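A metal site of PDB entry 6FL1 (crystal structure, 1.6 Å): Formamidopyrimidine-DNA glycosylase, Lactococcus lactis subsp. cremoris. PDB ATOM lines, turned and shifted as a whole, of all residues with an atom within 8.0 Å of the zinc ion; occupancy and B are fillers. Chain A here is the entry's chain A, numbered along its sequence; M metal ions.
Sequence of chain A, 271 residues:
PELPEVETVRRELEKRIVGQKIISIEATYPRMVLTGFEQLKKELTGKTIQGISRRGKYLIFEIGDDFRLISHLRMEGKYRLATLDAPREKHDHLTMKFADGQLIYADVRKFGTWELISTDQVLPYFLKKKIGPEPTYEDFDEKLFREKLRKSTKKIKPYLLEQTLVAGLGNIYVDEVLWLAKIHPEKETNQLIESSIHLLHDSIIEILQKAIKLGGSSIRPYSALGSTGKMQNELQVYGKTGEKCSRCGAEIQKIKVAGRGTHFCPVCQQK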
ATOM      1  N   TRP A 179     -28.957 -17.140 -27.280  1.00  0.00           N
ATOM      2  CA  TRP A 179     -27.639 -17.662 -26.921  1.00  0.00           C
ATOM      3  C   TRP A 179     -27.407 -17.583 -25.420  1.00  0.00           C
ATOM      4  O   TRP A 179     -26.939 -18.548 -24.798  1.00  0.00           O
ATOM      5  CB  TRP A 179     -26.549 -16.884 -27.667  1.00  0.00           C
ATOM      6  CG  TRP A 179     -25.144 -17.308 -27.299  1.00  0.00           C
ATOM      7  CD1 TRP A 179     -24.395 -18.272 -27.919  1.00  0.00           C
ATOM      8  CD2 TRP A 179     -24.316 -16.774 -26.256  1.00  0.00           C
ATOM      9  NE1 TRP A 179     -23.157 -18.366 -27.321  1.00  0.00           N
ATOM     10  CE2 TRP A 179     -23.089 -17.466 -26.304  1.00  0.00           C
ATOM     11  CE3 TRP A 179     -24.500 -15.793 -25.272  1.00  0.00           C
ATOM     12  CZ2 TRP A 179     -22.042 -17.193 -25.415  1.00  0.00           C
ATOM     13  CZ3 TRP A 179     -23.471 -15.535 -24.391  1.00  0.00           C
ATOM     14  CH2 TRP A 179     -22.256 -16.223 -24.471  1.00  0.00           C
ATOM     15  N   LYS A 182     -29.306 -20.225 -23.733  1.00  0.00           N
ATOM     16  CA  LYS A 182     -28.949 -21.582 -24.179  1.00  0.00           C
ATOM     17  C   LYS A 182     -30.154 -22.302 -24.789  1.00  0.00           C
ATOM     18  O   LYS A 182     -30.415 -23.479 -24.504  1.00  0.00           O
ATOM     19  CB  LYS A 182     -28.332 -22.382 -23.037  1.00  0.00           C
ATOM     20  CG  LYS A 182     -27.006 -21.764 -22.546  1.00  0.00           C
ATOM     21  CD  LYS A 182     -26.386 -22.566 -21.418  1.00  0.00           C
ATOM     22  CE  LYS A 182     -24.992 -22.062 -21.088  1.00  0.00           C
ATOM     23  NZ  LYS A 182     -24.176 -23.100 -20.380  1.00  0.00           N
ATOM     24  N   VAL A 237     -23.262 -13.410 -30.637  1.00  0.00           N
ATOM     25  CA  VAL A 237     -23.572 -14.248 -31.800  1.00  0.00           C
ATOM     26  C   VAL A 237     -23.994 -13.441 -33.025  1.00  0.00           C
ATOM     27  O   VAL A 237     -23.689 -13.839 -34.148  1.00  0.00           O
ATOM     28  CB  VAL A 237     -24.647 -15.293 -31.479  1.00  0.00           C
ATOM     29  CG1 VAL A 237     -24.084 -16.393 -30.598  1.00  0.00           C
ATOM     30  CG2 VAL A 237     -25.877 -14.659 -30.824  1.00  0.00           C
ATOM     31  N   LYS A 244     -15.677 -17.907 -32.858  1.00  0.00           N
ATOM     32  CA  LYS A 244     -15.850 -18.926 -31.828  1.00  0.00           C
ATOM     33  C   LYS A 244     -16.779 -18.448 -30.726  1.00  0.00           C
ATOM     34  O   LYS A 244     -16.732 -17.292 -30.303  1.00  0.00           O
ATOM     35  CB  LYS A 244     -14.498 -19.328 -31.239  1.00  0.00           C
ATOM     36  CG  LYS A 244     -13.452 -19.711 -32.274  1.00  0.00           C
ATOM     37  CD  LYS A 244     -13.930 -20.763 -33.275  1.00  0.00           C
ATOM     38  CE  LYS A 244     -12.775 -21.197 -34.177  1.00  0.00           C
ATOM     39  NZ  LYS A 244     -13.137 -22.154 -35.272  1.00  0.00           N
ATOM     40  N   CYS A 245     -17.649 -19.355 -30.279  1.00  0.00           N
ATOM     41  CA  CYS A 245     -18.482 -19.093 -29.114  1.00  0.00           C
ATOM     42  C   CYS A 245     -17.610 -18.790 -27.903  1.00  0.00           C
ATOM     43  O   CYS A 245     -16.651 -19.527 -27.616  1.00  0.00           O
ATOM     44  CB  CYS A 245     -19.382 -20.297 -28.844  1.00  0.00           C
ATOM     45  SG  CYS A 245     -20.337 -20.190 -27.330  1.00  0.00           S
ATOM     46  N   SER A 246     -17.924 -17.703 -27.194  1.00  0.00           N
ATOM     47  CA  SER A 246     -17.118 -17.317 -26.042  1.00  0.00           C
ATOM     48  C   SER A 246     -17.247 -18.290 -24.874  1.00  0.00           C
ATOM     49  O   SER A 246     -16.402 -18.268 -23.976  1.00  0.00           O
ATOM     50  CB  SER A 246     -17.512 -15.911 -25.577  1.00  0.00           C
ATOM     51  OG  SER A 246     -18.786 -15.938 -24.943  1.00  0.00           O
ATOM     52  N   ARG A 247     -18.264 -19.147 -24.869  1.00  0.00           N
ATOM     53  CA  ARG A 247     -18.439 -20.092 -23.767  1.00  0.00           C
ATOM     54  C   ARG A 247     -17.748 -21.429 -24.025  1.00  0.00           C
ATOM     55  O   ARG A 247     -17.040 -21.939 -23.155  1.00  0.00           O
ATOM     56  CB  ARG A 247     -19.930 -20.317 -23.491  1.00  0.00           C
ATOM     57  CG  ARG A 247     -20.548 -19.260 -22.580  1.00  0.00           C
ATOM     58  CD  ARG A 247     -22.005 -19.586 -22.210  1.00  0.00           C
ATOM     59  NE  ARG A 247     -22.779 -19.912 -23.398  1.00  0.00           N
ATOM     60  CZ  ARG A 247     -24.024 -19.543 -23.615  1.00  0.00           C
ATOM     61  NH1 ARG A 247     -24.689 -18.821 -22.700  1.00  0.00           N
ATOM     62  NH2 ARG A 247     -24.636 -19.883 -24.734  1.00  0.00           N
ATOM     63  N   CYS A 248     -17.930 -21.991 -25.216  1.00  0.00           N
ATOM     64  CA  CYS A 248     -17.488 -23.356 -25.490  1.00  0.00           C
ATOM     65  C   CYS A 248     -16.481 -23.478 -26.618  1.00  0.00           C
ATOM     66  O   CYS A 248     -15.909 -24.563 -26.796  1.00  0.00           O
ATOM     67  CB  CYS A 248     -18.700 -24.241 -25.831  1.00  0.00           C
ATOM     68  SG  CYS A 248     -19.400 -23.905 -27.447  1.00  0.00           S
ATOM     69  N   GLY A 249     -16.242 -22.413 -27.389  1.00  0.00           N
ATOM     70  CA  GLY A 249     -15.290 -22.455 -28.462  1.00  0.00           C
ATOM     71  C   GLY A 249     -15.799 -22.994 -29.784  1.00  0.00           C
ATOM     72  O   GLY A 249     -15.036 -23.004 -30.759  1.00  0.00           O
ATOM     73  N   ALA A 250     -17.051 -23.447 -29.856  1.00  0.00           N
ATOM     74  CA  ALA A 250     -17.587 -23.882 -31.132  1.00  0.00           C
ATOM     75  C   ALA A 250     -17.814 -22.697 -32.064  1.00  0.00           C
ATOM     76  O   ALA A 250     -18.056 -21.573 -31.606  1.00  0.00           O
ATOM     77  CB  ALA A 250     -18.905 -24.638 -30.924  1.00  0.00           C
ATOM     78  N   GLU A 251     -17.755 -22.952 -33.365  1.00  0.00           N
ATOM     79  CA  GLU A 251     -17.997 -21.878 -34.336  1.00  0.00           C
ATOM     80  C   GLU A 251     -19.466 -21.478 -34.343  1.00  0.00           C
ATOM     81  O   GLU A 251     -20.354 -22.337 -34.417  1.00  0.00           O
ATOM     82  CB  GLU A 251     -17.573 -22.303 -35.747  1.00  0.00           C
ATOM     83  CG  GLU A 251     -16.127 -22.051 -36.022  1.00  0.00           C
ATOM     84  CD  GLU A 251     -15.758 -22.037 -37.493  1.00  0.00           C
ATOM     85  OE1 GLU A 251     -16.651 -21.972 -38.381  1.00  0.00           O
ATOM     86  OE2 GLU A 251     -14.550 -22.055 -37.754  1.00  0.00           O
ATOM     87  N   ILE A 252     -19.721 -20.174 -34.293  1.00  0.00           N
ATOM     88  CA  ILE A 252     -21.075 -19.666 -34.442  1.00  0.00           C
ATOM     89  C   ILE A 252     -21.564 -19.946 -35.859  1.00  0.00           C
ATOM     90  O   ILE A 252     -20.848 -19.690 -36.849  1.00  0.00           O
ATOM     91  CB  ILE A 252     -21.116 -18.155 -34.126  1.00  0.00           C
ATOM     92  CG1 ILE A 252     -20.661 -17.918 -32.676  1.00  0.00           C
ATOM     93  CG2 ILE A 252     -22.502 -17.584 -34.404  1.00  0.00           C
ATOM     94  CD1 ILE A 252     -21.420 -18.727 -31.628  1.00  0.00           C
ATOM     95  N   PHE A 264     -26.320 -18.652 -33.997  1.00  0.00           N
ATOM     96  CA  PHE A 264     -26.433 -19.438 -32.771  1.00  0.00           C
ATOM     97  C   PHE A 264     -25.178 -20.297 -32.594  1.00  0.00           C
ATOM     98  O   PHE A 264     -24.438 -20.547 -33.544  1.00  0.00           O
ATOM     99  CB  PHE A 264     -27.678 -20.336 -32.791  1.00  0.00           C
ATOM    100  CG  PHE A 264     -27.562 -21.489 -33.751  1.00  0.00           C
ATOM    101  CD1 PHE A 264     -27.614 -21.263 -35.123  1.00  0.00           C
ATOM    102  CD2 PHE A 264     -27.353 -22.770 -33.292  1.00  0.00           C
ATOM    103  CE1 PHE A 264     -27.474 -22.316 -36.018  1.00  0.00           C
ATOM    104  CE2 PHE A 264     -27.217 -23.828 -34.180  1.00  0.00           C
ATOM    105  CZ  PHE A 264     -27.282 -23.602 -35.548  1.00  0.00           C
ATOM    106  N   CYS A 265     -24.952 -20.731 -31.359  1.00  0.00           N
ATOM    107  CA  CYS A 265     -23.913 -21.716 -31.092  1.00  0.00           C
ATOM    108  C   CYS A 265     -24.546 -23.105 -31.073  1.00  0.00           C
ATOM    109  O   CYS A 265     -25.441 -23.345 -30.244  1.00  0.00           O
ATOM    110  CB  CYS A 265     -23.224 -21.465 -29.765  1.00  0.00           C
ATOM    111  SG  CYS A 265     -22.112 -22.829 -29.308  1.00  0.00           S
ATOM    112  N   PRO A 266     -24.137 -24.025 -31.940  1.00  0.00           N
ATOM    113  CA  PRO A 266     -24.772 -25.361 -31.969  1.00  0.00           C
ATOM    114  C   PRO A 266     -24.487 -26.202 -30.747  1.00  0.00           C
ATOM    115  O   PRO A 266     -25.189 -27.202 -30.558  1.00  0.00           O
ATOM    116  CB  PRO A 266     -24.185 -26.022 -33.220  1.00  0.00           C
ATOM    117  CG  PRO A 266     -23.514 -24.930 -33.962  1.00  0.00           C
ATOM    118  CD  PRO A 266     -23.119 -23.872 -32.985  1.00  0.00           C
ATOM    119  N   VAL A 267     -23.473 -25.870 -29.950  1.00  0.00           N
ATOM    120  CA  VAL A 267     -23.194 -26.617 -28.727  1.00  0.00           C
ATOM    121  C   VAL A 267     -24.040 -26.093 -27.582  1.00  0.00           C
ATOM    122  O   VAL A 267     -24.736 -26.855 -26.893  1.00  0.00           O
ATOM    123  CB  VAL A 267     -21.691 -26.549 -28.394  1.00  0.00           C
ATOM    124  CG1 VAL A 267     -21.439 -27.157 -27.022  1.00  0.00           C
ATOM    125  CG2 VAL A 267     -20.874 -27.316 -29.426  1.00  0.00           C
ATOM    126  N   CYS A 268     -23.983 -24.775 -27.361  1.00  0.00           N
ATOM    127  CA  CYS A 268     -24.709 -24.176 -26.240  1.00  0.00           C
ATOM    128  C   CYS A 268     -26.214 -24.164 -26.458  1.00  0.00           C
ATOM    129  O   CYS A 268     -26.971 -24.084 -25.489  1.00  0.00           O
ATOM    130  CB  CYS A 268     -24.230 -22.745 -26.025  1.00  0.00           C
ATOM    131  SG  CYS A 268     -22.529 -22.612 -25.442  1.00  0.00           S
ATOM    132  N   GLN A 269     -26.678 -24.186 -27.712  1.00  0.00           N
ATOM    133  CA  GLN A 269     -28.096 -24.081 -28.044  1.00  0.00           C
ATOM    134  C   GLN A 269     -28.489 -25.360 -28.769  1.00  0.00           C
ATOM    135  O   GLN A 269     -28.563 -25.397 -30.008  1.00  0.00           O
ATOM    136  CB  GLN A 269     -28.389 -22.830 -28.871  1.00  0.00           C
ATOM    137  CG  GLN A 269     -28.006 -21.553 -28.156  1.00  0.00           C
ATOM    138  CD  GLN A 269     -27.955 -20.361 -29.091  1.00  0.00           C
ATOM    139  OE1 GLN A 269     -26.874 -19.958 -29.524  1.00  0.00           O
ATOM    140  NE2 GLN A 269     -29.111 -19.798 -29.399  1.00  0.00           N
HETATM  141 ZN    ZN M   1     -21.120 -22.363 -27.288  1.00  0.00          ZN
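Of the 18 residues printed, 4 come within 4 Å of the zinc ion.
Along chain A the residues within 4 Å of the zinc ion span positions 245 to 268.
The nearest printed residue that does not touch the zinc ion is Val 267 (4.4 Å).
The zinc ion is bound by SG of Cys 265, at 2.3 Å.
The zinc ion is bound by the side-chain sulfur (SG) of Cys 245 (2.3 Å).
The zinc ion is bound by SG of Cys 248.
The zinc ion is bound by SG of Cys 268, 2.3 Å away.
The backbone NH (N) of Cys 245 sits at hydrogen-bond distance from the backbone carbonyl oxygen (O) of Ala 250 (2.6 Å).
SG of Cys 248 lies close to N of Ala 250, 3.4 Å away.
The side-chain sulfur of Cys 265 sits close to the backbone NH of Val 267 (3.4 Å).
NE1 of Trp 179 lies close to SG of Cys 245 (3.4 Å).
The side-chain amide oxygen (OE1) of Gln 269 is in hydrogen-bond range of the backbone NH (N) of Cys 265, 2.8 Å away.
SG of Cys 268 sits close to NE of Arg 247 (3.4 Å).
SG of Cys 245 lies close to N of Arg 247 (3.4 Å).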
